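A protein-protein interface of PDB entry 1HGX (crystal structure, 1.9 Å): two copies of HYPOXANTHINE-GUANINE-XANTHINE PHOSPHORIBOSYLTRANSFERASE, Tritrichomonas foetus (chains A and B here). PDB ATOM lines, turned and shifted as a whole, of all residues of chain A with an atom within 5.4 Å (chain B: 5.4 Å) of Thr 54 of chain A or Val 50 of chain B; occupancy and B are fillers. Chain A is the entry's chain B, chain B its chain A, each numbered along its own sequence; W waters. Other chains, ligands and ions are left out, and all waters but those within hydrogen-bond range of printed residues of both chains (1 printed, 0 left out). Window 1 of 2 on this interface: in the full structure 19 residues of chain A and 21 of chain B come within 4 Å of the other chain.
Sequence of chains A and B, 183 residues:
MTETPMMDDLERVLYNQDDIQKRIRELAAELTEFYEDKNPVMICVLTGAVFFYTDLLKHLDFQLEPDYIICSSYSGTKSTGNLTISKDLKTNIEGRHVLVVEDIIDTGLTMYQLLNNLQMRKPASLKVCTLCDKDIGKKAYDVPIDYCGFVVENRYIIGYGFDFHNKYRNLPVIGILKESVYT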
ATOM      1  N   ALA A  49      -3.048  25.792 -10.412  1.00  0.00           N
ATOM      2  CA  ALA A  49      -1.980  25.489  -9.458  1.00  0.00           C
ATOM      3  C   ALA A  49      -1.999  24.122  -8.740  1.00  0.00           C
ATOM      4  O   ALA A  49      -1.006  23.752  -8.109  1.00  0.00           O
ATOM      5  CB  ALA A  49      -1.889  26.612  -8.435  1.00  0.00           C
ATOM      6  N   VAL A  50      -3.068  23.345  -8.912  1.00  0.00           N
ATOM      7  CA  VAL A  50      -3.228  22.049  -8.229  1.00  0.00           C
ATOM      8  C   VAL A  50      -2.067  21.029  -8.240  1.00  0.00           C
ATOM      9  O   VAL A  50      -1.731  20.476  -7.193  1.00  0.00           O
ATOM     10  CB  VAL A  50      -4.555  21.347  -8.641  1.00  0.00           C
ATOM     11  CG1 VAL A  50      -4.802  20.145  -7.755  1.00  0.00           C
ATOM     12  CG2 VAL A  50      -5.727  22.307  -8.505  1.00  0.00           C
ATOM     13  N   PHE A  51      -1.472  20.764  -9.399  1.00  0.00           N
ATOM     14  CA  PHE A  51      -0.364  19.808  -9.497  1.00  0.00           C
ATOM     15  C   PHE A  51       0.809  20.258  -8.623  1.00  0.00           C
ATOM     16  O   PHE A  51       1.354  19.493  -7.829  1.00  0.00           O
ATOM     17  CB  PHE A  51       0.118  19.699 -10.953  1.00  0.00           C
ATOM     18  CG  PHE A  51      -0.543  18.604 -11.748  1.00  0.00           C
ATOM     19  CD1 PHE A  51      -1.927  18.532 -11.861  1.00  0.00           C
ATOM     20  CD2 PHE A  51       0.228  17.642 -12.390  1.00  0.00           C
ATOM     21  CE1 PHE A  51      -2.535  17.513 -12.603  1.00  0.00           C
ATOM     22  CE2 PHE A  51      -0.368  16.624 -13.131  1.00  0.00           C
ATOM     23  CZ  PHE A  51      -1.750  16.560 -13.237  1.00  0.00           C
ATOM     24  N   PHE A  52       1.181  21.521  -8.796  1.00  0.00           N
ATOM     25  CA  PHE A  52       2.277  22.165  -8.075  1.00  0.00           C
ATOM     26  C   PHE A  52       1.985  22.200  -6.580  1.00  0.00           C
ATOM     27  O   PHE A  52       2.840  21.868  -5.756  1.00  0.00           O
ATOM     28  CB  PHE A  52       2.430  23.598  -8.605  1.00  0.00           C
ATOM     29  CG  PHE A  52       3.511  24.403  -7.929  1.00  0.00           C
ATOM     30  CD1 PHE A  52       4.753  23.843  -7.647  1.00  0.00           C
ATOM     31  CD2 PHE A  52       3.297  25.743  -7.624  1.00  0.00           C
ATOM     32  CE1 PHE A  52       5.758  24.611  -7.076  1.00  0.00           C
ATOM     33  CE2 PHE A  52       4.300  26.514  -7.056  1.00  0.00           C
ATOM     34  CZ  PHE A  52       5.529  25.951  -6.783  1.00  0.00           C
ATOM     35  N   TYR A  53       0.768  22.614  -6.253  1.00  0.00           N
ATOM     36  CA  TYR A  53       0.312  22.733  -4.881  1.00  0.00           C
ATOM     37  C   TYR A  53       0.452  21.429  -4.095  1.00  0.00           C
ATOM     38  O   TYR A  53       1.070  21.410  -3.022  1.00  0.00           O
ATOM     39  CB  TYR A  53      -1.143  23.200  -4.876  1.00  0.00           C
ATOM     40  CG  TYR A  53      -1.714  23.488  -3.511  1.00  0.00           C
ATOM     41  CD1 TYR A  53      -1.359  24.640  -2.819  1.00  0.00           C
ATOM     42  CD2 TYR A  53      -2.657  22.637  -2.937  1.00  0.00           C
ATOM     43  CE1 TYR A  53      -1.934  24.947  -1.590  1.00  0.00           C
ATOM     44  CE2 TYR A  53      -3.240  22.932  -1.706  1.00  0.00           C
ATOM     45  CZ  TYR A  53      -2.878  24.091  -1.039  1.00  0.00           C
ATOM     46  OH  TYR A  53      -3.476  24.406   0.161  1.00  0.00           O
ATOM     47  N   THR A  54      -0.079  20.337  -4.643  1.00  0.00           N
ATOM     48  CA  THR A  54      -0.014  19.037  -3.966  1.00  0.00           C
ATOM     49  C   THR A  54       1.415  18.511  -3.871  1.00  0.00           C
ATOM     50  O   THR A  54       1.783  17.878  -2.878  1.00  0.00           O
ATOM     51  CB  THR A  54      -0.885  17.985  -4.664  1.00  0.00           C
ATOM     52  OG1 THR A  54      -0.298  17.655  -5.924  1.00  0.00           O
ATOM     53  CG2 THR A  54      -2.271  18.535  -4.912  1.00  0.00           C
ATOM     54  N   ASP A  55       2.219  18.750  -4.907  1.00  0.00           N
ATOM     55  CA  ASP A  55       3.613  18.308  -4.886  1.00  0.00           C
ATOM     56  C   ASP A  55       4.388  19.057  -3.820  1.00  0.00           C
ATOM     57  O   ASP A  55       5.304  18.501  -3.220  1.00  0.00           O
ATOM     58  CB  ASP A  55       4.278  18.453  -6.256  1.00  0.00           C
ATOM     59  CG  ASP A  55       4.055  17.239  -7.139  1.00  0.00           C
ATOM     60  OD1 ASP A  55       3.680  16.171  -6.605  1.00  0.00           O
ATOM     61  OD2 ASP A  55       4.250  17.347  -8.367  1.00  0.00           O
ATOM     62  N   LEU A  56       4.016  20.310  -3.577  1.00  0.00           N
ATOM     63  CA  LEU A  56       4.657  21.096  -2.528  1.00  0.00           C
ATOM     64  C   LEU A  56       4.223  20.544  -1.170  1.00  0.00           C
ATOM     65  O   LEU A  56       5.049  20.288  -0.298  1.00  0.00           O
ATOM     66  CB  LEU A  56       4.224  22.557  -2.602  1.00  0.00           C
ATOM     67  CG  LEU A  56       5.062  23.601  -3.331  1.00  0.00           C
ATOM     68  CD1 LEU A  56       4.350  24.930  -3.173  1.00  0.00           C
ATOM     69  CD2 LEU A  56       6.469  23.677  -2.736  1.00  0.00           C
ATOM     70  N   LEU A  57       2.917  20.348  -1.003  1.00  0.00           N
ATOM     71  CA  LEU A  57       2.372  19.846   0.253  1.00  0.00           C
ATOM     72  C   LEU A  57       2.933  18.485   0.651  1.00  0.00           C
ATOM     73  O   LEU A  57       2.941  18.133   1.832  1.00  0.00           O
ATOM     74  CB  LEU A  57       0.844  19.831   0.222  1.00  0.00           C
ATOM     75  CG  LEU A  57       0.198  21.046   0.898  1.00  0.00           C
ATOM     76  CD1 LEU A  57       0.602  22.355   0.235  1.00  0.00           C
ATOM     77  CD2 LEU A  57      -1.299  20.879   0.870  1.00  0.00           C
ATOM     78  N   LYS A  58       3.456  17.744  -0.322  1.00  0.00           N
ATOM     79  CA  LYS A  58       4.048  16.440  -0.036  1.00  0.00           C
ATOM     80  C   LYS A  58       5.382  16.589   0.692  1.00  0.00           C
ATOM     81  O   LYS A  58       5.914  15.617   1.205  1.00  0.00           O
ATOM     82  CB  LYS A  58       4.260  15.647  -1.323  1.00  0.00           C
ATOM     83  CG  LYS A  58       2.978  15.244  -1.992  1.00  0.00           C
ATOM     84  CD  LYS A  58       3.236  14.410  -3.231  1.00  0.00           C
ATOM     85  CE  LYS A  58       1.927  14.031  -3.920  1.00  0.00           C
ATOM     86  NZ  LYS A  58       2.155  13.165  -5.104  1.00  0.00           N
ATOM     87  N   TYR A  68      -8.803  27.554  -0.893  1.00  0.00           N
ATOM     88  CA  TYR A  68      -8.822  27.637  -2.335  1.00  0.00           C
ATOM     89  C   TYR A  68      -9.548  28.882  -2.786  1.00  0.00           C
ATOM     90  O   TYR A  68     -10.433  29.387  -2.087  1.00  0.00           O
ATOM     91  CB  TYR A  68      -9.506  26.386  -2.895  1.00  0.00           C
ATOM     92  CG  TYR A  68      -8.888  25.114  -2.370  1.00  0.00           C
ATOM     93  CD1 TYR A  68      -9.288  24.575  -1.144  1.00  0.00           C
ATOM     94  CD2 TYR A  68      -7.850  24.491  -3.057  1.00  0.00           C
ATOM     95  CE1 TYR A  68      -8.658  23.452  -0.615  1.00  0.00           C
ATOM     96  CE2 TYR A  68      -7.216  23.369  -2.537  1.00  0.00           C
ATOM     97  CZ  TYR A  68      -7.623  22.857  -1.318  1.00  0.00           C
ATOM     98  OH  TYR A  68      -6.985  21.756  -0.803  1.00  0.00           O
ATOM     99  N   CYS B  44     -12.902  16.331  -7.978  1.00  0.00           N
ATOM    100  CA  CYS B  44     -12.077  16.041  -6.826  1.00  0.00           C
ATOM    101  C   CYS B  44     -12.766  16.651  -5.600  1.00  0.00           C
ATOM    102  O   CYS B  44     -13.117  17.845  -5.597  1.00  0.00           O
ATOM    103  CB  CYS B  44     -10.690  16.664  -6.994  1.00  0.00           C
ATOM    104  SG  CYS B  44      -9.653  16.581  -5.524  1.00  0.00           S
ATOM    105  N   VAL B  45     -13.017  15.830  -4.586  1.00  0.00           N
ATOM    106  CA  VAL B  45     -13.628  16.327  -3.358  1.00  0.00           C
ATOM    107  C   VAL B  45     -12.456  16.764  -2.467  1.00  0.00           C
ATOM    108  O   VAL B  45     -11.728  15.936  -1.906  1.00  0.00           O
ATOM    109  CB  VAL B  45     -14.488  15.241  -2.663  1.00  0.00           C
ATOM    110  CG1 VAL B  45     -15.127  15.812  -1.391  1.00  0.00           C
ATOM    111  CG2 VAL B  45     -15.571  14.701  -3.638  1.00  0.00           C
ATOM    112  N   LEU B  46     -12.246  18.076  -2.402  1.00  0.00           N
ATOM    113  CA  LEU B  46     -11.147  18.660  -1.632  1.00  0.00           C
ATOM    114  C   LEU B  46     -11.415  18.562  -0.141  1.00  0.00           C
ATOM    115  O   LEU B  46     -12.575  18.547   0.264  1.00  0.00           O
ATOM    116  CB  LEU B  46     -10.963  20.118  -2.023  1.00  0.00           C
ATOM    117  CG  LEU B  46     -10.566  20.357  -3.476  1.00  0.00           C
ATOM    118  CD1 LEU B  46     -10.833  21.801  -3.840  1.00  0.00           C
ATOM    119  CD2 LEU B  46      -9.111  19.992  -3.678  1.00  0.00           C
ATOM    120  N   THR B  47     -10.376  18.476   0.688  1.00  0.00           N
ATOM    121  CA  THR B  47      -8.970  18.488   0.293  1.00  0.00           C
ATOM    122  C   THR B  47      -8.325  17.109   0.243  1.00  0.00           C
ATOM    123  O   THR B  47      -7.511  16.836  -0.633  1.00  0.00           O
ATOM    124  CB  THR B  47      -8.142  19.334   1.313  1.00  0.00           C
ATOM    125  OG1 THR B  47      -8.564  20.696   1.261  1.00  0.00           O
ATOM    126  CG2 THR B  47      -6.647  19.249   1.049  1.00  0.00           C
ATOM    127  N   GLY B  48      -8.664  16.265   1.213  1.00  0.00           N
ATOM    128  CA  GLY B  48      -8.079  14.934   1.321  1.00  0.00           C
ATOM    129  C   GLY B  48      -7.805  14.131   0.065  1.00  0.00           C
ATOM    130  O   GLY B  48      -6.756  13.495  -0.054  1.00  0.00           O
ATOM    131  N   ALA B  49      -8.740  14.163  -0.878  1.00  0.00           N
ATOM    132  CA  ALA B  49      -8.604  13.411  -2.121  1.00  0.00           C
ATOM    133  C   ALA B  49      -7.631  14.021  -3.135  1.00  0.00           C
ATOM    134  O   ALA B  49      -7.259  13.364  -4.107  1.00  0.00           O
ATOM    135  CB  ALA B  49      -9.979  13.237  -2.762  1.00  0.00           C
ATOM    136  N   VAL B  50      -7.164  15.241  -2.882  1.00  0.00           N
ATOM    137  CA  VAL B  50      -6.293  15.925  -3.832  1.00  0.00           C
ATOM    138  C   VAL B  50      -4.986  15.218  -4.205  1.00  0.00           C
ATOM    139  O   VAL B  50      -4.591  15.243  -5.370  1.00  0.00           O
ATOM    140  CB  VAL B  50      -6.063  17.409  -3.433  1.00  0.00           C
ATOM    141  CG1 VAL B  50      -5.013  17.540  -2.347  1.00  0.00           C
ATOM    142  CG2 VAL B  50      -5.734  18.248  -4.668  1.00  0.00           C
ATOM    143  N   PHE B  51      -4.345  14.545  -3.251  1.00  0.00           N
ATOM    144  CA  PHE B  51      -3.096  13.847  -3.539  1.00  0.00           C
ATOM    145  C   PHE B  51      -3.390  12.711  -4.496  1.00  0.00           C
ATOM    146  O   PHE B  51      -2.765  12.594  -5.539  1.00  0.00           O
ATOM    147  CB  PHE B  51      -2.466  13.302  -2.256  1.00  0.00           C
ATOM    148  CG  PHE B  51      -1.850  14.362  -1.389  1.00  0.00           C
ATOM    149  CD1 PHE B  51      -2.604  15.434  -0.930  1.00  0.00           C
ATOM    150  CD2 PHE B  51      -0.513  14.294  -1.036  1.00  0.00           C
ATOM    151  CE1 PHE B  51      -2.034  16.431  -0.131  1.00  0.00           C
ATOM    152  CE2 PHE B  51       0.067  15.287  -0.236  1.00  0.00           C
ATOM    153  CZ  PHE B  51      -0.701  16.356   0.215  1.00  0.00           C
ATOM    154  N   PHE B  52      -4.362  11.888  -4.120  1.00  0.00           N
ATOM    155  CA  PHE B  52      -4.822  10.750  -4.902  1.00  0.00           C
ATOM    156  C   PHE B  52      -5.255  11.215  -6.289  1.00  0.00           C
ATOM    157  O   PHE B  52      -4.900  10.600  -7.298  1.00  0.00           O
ATOM    158  CB  PHE B  52      -6.011  10.118  -4.171  1.00  0.00           C
ATOM    159  CG  PHE B  52      -6.704   9.022  -4.928  1.00  0.00           C
ATOM    160  CD1 PHE B  52      -5.979   8.009  -5.553  1.00  0.00           C
ATOM    161  CD2 PHE B  52      -8.099   8.969  -4.961  1.00  0.00           C
ATOM    162  CE1 PHE B  52      -6.631   6.943  -6.184  1.00  0.00           C
ATOM    163  CE2 PHE B  52      -8.769   7.905  -5.590  1.00  0.00           C
ATOM    164  CZ  PHE B  52      -8.034   6.893  -6.204  1.00  0.00           C
ATOM    165  N   TYR B  53      -6.001  12.317  -6.322  1.00  0.00           N
ATOM    166  CA  TYR B  53      -6.531  12.902  -7.559  1.00  0.00           C
ATOM    167  C   TYR B  53      -5.435  13.318  -8.537  1.00  0.00           C
ATOM    168  O   TYR B  53      -5.453  12.912  -9.707  1.00  0.00           O
ATOM    169  CB  TYR B  53      -7.412  14.109  -7.227  1.00  0.00           C
ATOM    170  CG  TYR B  53      -8.085  14.775  -8.416  1.00  0.00           C
ATOM    171  CD1 TYR B  53      -9.242  14.236  -8.980  1.00  0.00           C
ATOM    172  CD2 TYR B  53      -7.610  15.988  -8.925  1.00  0.00           C
ATOM    173  CE1 TYR B  53      -9.918  14.893 -10.016  1.00  0.00           C
ATOM    174  CE2 TYR B  53      -8.281  16.652  -9.961  1.00  0.00           C
ATOM    175  CZ  TYR B  53      -9.433  16.098 -10.497  1.00  0.00           C
ATOM    176  OH  TYR B  53     -10.106  16.760 -11.508  1.00  0.00           O
ATOM    177  N   THR B  54      -4.488  14.130  -8.080  1.00  0.00           N
ATOM    178  CA  THR B  54      -3.417  14.561  -8.966  1.00  0.00           C
ATOM    179  C   THR B  54      -2.543  13.392  -9.422  1.00  0.00           C
ATOM    180  O   THR B  54      -2.078  13.377 -10.563  1.00  0.00           O
ATOM    181  CB  THR B  54      -2.552  15.650  -8.324  1.00  0.00           C
ATOM    182  OG1 THR B  54      -1.968  15.141  -7.125  1.00  0.00           O
ATOM    183  CG2 THR B  54      -3.401  16.877  -7.999  1.00  0.00           C
ATOM    184  N   ASP B  55      -2.321  12.412  -8.548  1.00  0.00           N
ATOM    185  CA  ASP B  55      -1.508  11.252  -8.927  1.00  0.00           C
ATOM    186  C   ASP B  55      -2.181  10.441 -10.024  1.00  0.00           C
ATOM    187  O   ASP B  55      -1.511   9.944 -10.936  1.00  0.00           O
ATOM    188  CB  ASP B  55      -1.189  10.371  -7.718  1.00  0.00           C
ATOM    189  CG  ASP B  55       0.023  10.870  -6.936  1.00  0.00           C
ATOM    190  OD1 ASP B  55       0.751  11.753  -7.439  1.00  0.00           O
ATOM    191  OD2 ASP B  55       0.256  10.381  -5.813  1.00  0.00           O
ATOM    192  N   LYS B  58      -1.982  12.185 -13.448  1.00  0.00           N
ATOM    193  CA  LYS B  58      -0.661  12.095 -14.062  1.00  0.00           C
ATOM    194  C   LYS B  58      -0.556  10.838 -14.926  1.00  0.00           C
ATOM    195  O   LYS B  58       0.391  10.680 -15.696  1.00  0.00           O
ATOM    196  CB  LYS B  58       0.433  12.080 -12.998  1.00  0.00           C
ATOM    197  CG  LYS B  58       0.635  13.406 -12.330  1.00  0.00           C
ATOM    198  CD  LYS B  58       1.542  13.254 -11.145  1.00  0.00           C
ATOM    199  CE  LYS B  58       1.676  14.563 -10.401  1.00  0.00           C
ATOM    200  NZ  LYS B  58       2.336  14.331  -9.093  1.00  0.00           N
ATOM    201  N   TYR B  68     -13.851  20.774  -9.012  1.00  0.00           N
ATOM    202  CA  TYR B  68     -13.660  20.571  -7.585  1.00  0.00           C
ATOM    203  C   TYR B  68     -14.871  20.924  -6.777  1.00  0.00           C
ATOM    204  O   TYR B  68     -15.626  21.821  -7.138  1.00  0.00           O
ATOM    205  CB  TYR B  68     -12.497  21.445  -7.113  1.00  0.00           C
ATOM    206  CG  TYR B  68     -11.239  21.188  -7.896  1.00  0.00           C
ATOM    207  CD1 TYR B  68     -11.018  21.819  -9.118  1.00  0.00           C
ATOM    208  CD2 TYR B  68     -10.318  20.239  -7.462  1.00  0.00           C
ATOM    209  CE1 TYR B  68      -9.917  21.499  -9.894  1.00  0.00           C
ATOM    210  CE2 TYR B  68      -9.213  19.911  -8.228  1.00  0.00           C
ATOM    211  CZ  TYR B  68      -9.022  20.540  -9.445  1.00  0.00           C
ATOM    212  OH  TYR B  68      -7.959  20.176 -10.234  1.00  0.00           O
HETATM  213  O   HOH W   1       3.025  10.524  -4.450  1.00  0.00           O
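OG1 of Thr 47 of chain B sits at hydrogen-bond distance from OH of Tyr 68 of chain A, at 2.8 Å.
OG1 of Thr 54 of chain B lies within hydrogen-bond range of OG1 of Thr 54 of chain A, 3.2 Å away.
The side-chain amino group (NZ) of Lys 58 of chain A is in salt-bridge range of the side-chain carboxylate (OD1) of Asp 55 of chain B (3.1 Å).
OD1 of Asp 55 of chain A lies within salt-bridge range of NZ of Lys 58 of chain B (3.4 Å).
The backbone carbonyl oxygen (O) of Val 50 of chain B lies within hydrogen-bond range of the side-chain hydroxyl (OG1) of Thr 54 of chain B, at 3.2 Å.
O of Phe 51 of chain B sits at hydrogen-bond distance from OG1 of Thr 54 of chain B.
The side-chain carboxylate (OD1) of Asp 55 of chain B lies within salt-bridge range of the side-chain amino group (NZ) of Lys 58 of chain B.
The side-chain hydroxyl (OG1) of Thr 54 of chain A lies close to the backbone carbonyl oxygen (O) of Val 50 of chain A (3.4 Å).
The backbone carbonyl oxygen of Phe 51 of chain A sits at hydrogen-bond distance from the side-chain hydroxyl of Thr 54 of chain A (3.1 Å).
OD1 of Asp 55 of chain A is in salt-bridge range of NZ of Lys 58 of chain A.
Among the printed residues, merely in contact across the chains: Val 50 of chain A with Val 50 of chain B (3.7 Å), Val 50 of chain A with Thr 54 of chain B (3.6 Å), Val 50 of chain A with Tyr 68 of chain B (3.5 Å), Phe 51 of chain A with Lys 58 of chain B (3.5 Å), Thr 54 of chain A with Val 50 of chain B (3.5 Å), Leu 57 of chain A with Phe 51 of chain B (3.8 Å), Lys 58 of chain A with Phe 51 of chain B (3.4 Å) and Tyr 68 of chain A with Leu 46 of chain B (3.99 Å).
Of the printed residues of chain B, Phe 51 of chain A touches Lys 58.
Tyr 53 of chain A touches none of the printed residues of chain B.
Thr 54 of chain A touches just these residues of chain B: Val 50 (3.5 Å) and Thr 54 (3.2 Å).
Of the printed residues of chain B, Asp 55 of chain A touches Lys 58.
Of chain A, only Val 50 (3.7 Å) and Thr 54 (3.5 Å) come within 4 Å of Val 50 of chain B.
Printed residues of chain A within 4 Å of Phe 51 of chain B: Leu 57 and Lys 58.
The nearest residue of chain A that does not touch Val 50 of chain B is Tyr 68 of chain A (4.9 Å).
Printed residues of chain A that touch a printed residue of chain B: Val 50, Phe 51, Thr 54, Asp 55, Leu 57, Lys 58 and Tyr 68.
Hydrophobic or aromatic side chains of chain A that line the printed part of chain B: Val 50, Phe 51, Leu 57 and Tyr 68.
Val 50 of chain A touches its own counterpart, Val 50 of chain B.
Val 50 of chain A touches Tyr 68 of chain B, but with the chains exchanged Tyr 68 of chain A does not touch Val 50 of chain B (4.9 Å).
Phe 51 of chain A touches Lys 58 of chain B, and with the chains exchanged Lys 58 of chain A touches Phe 51 of chain B.
Thr 54 of chain B touches its own counterpart, Thr 54 of chain A.
Positions printed for both chains: 49, 50, 51, 52, 53, 54, 55, 58 and 68.
Of the 12 pairs that touch across the chains among the printed residues, 8 have their exchanged pair printed and touching as well.
Water W1 bridges NZ of Lys 58 of chain A and OD2 of Asp 55 of chain B.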
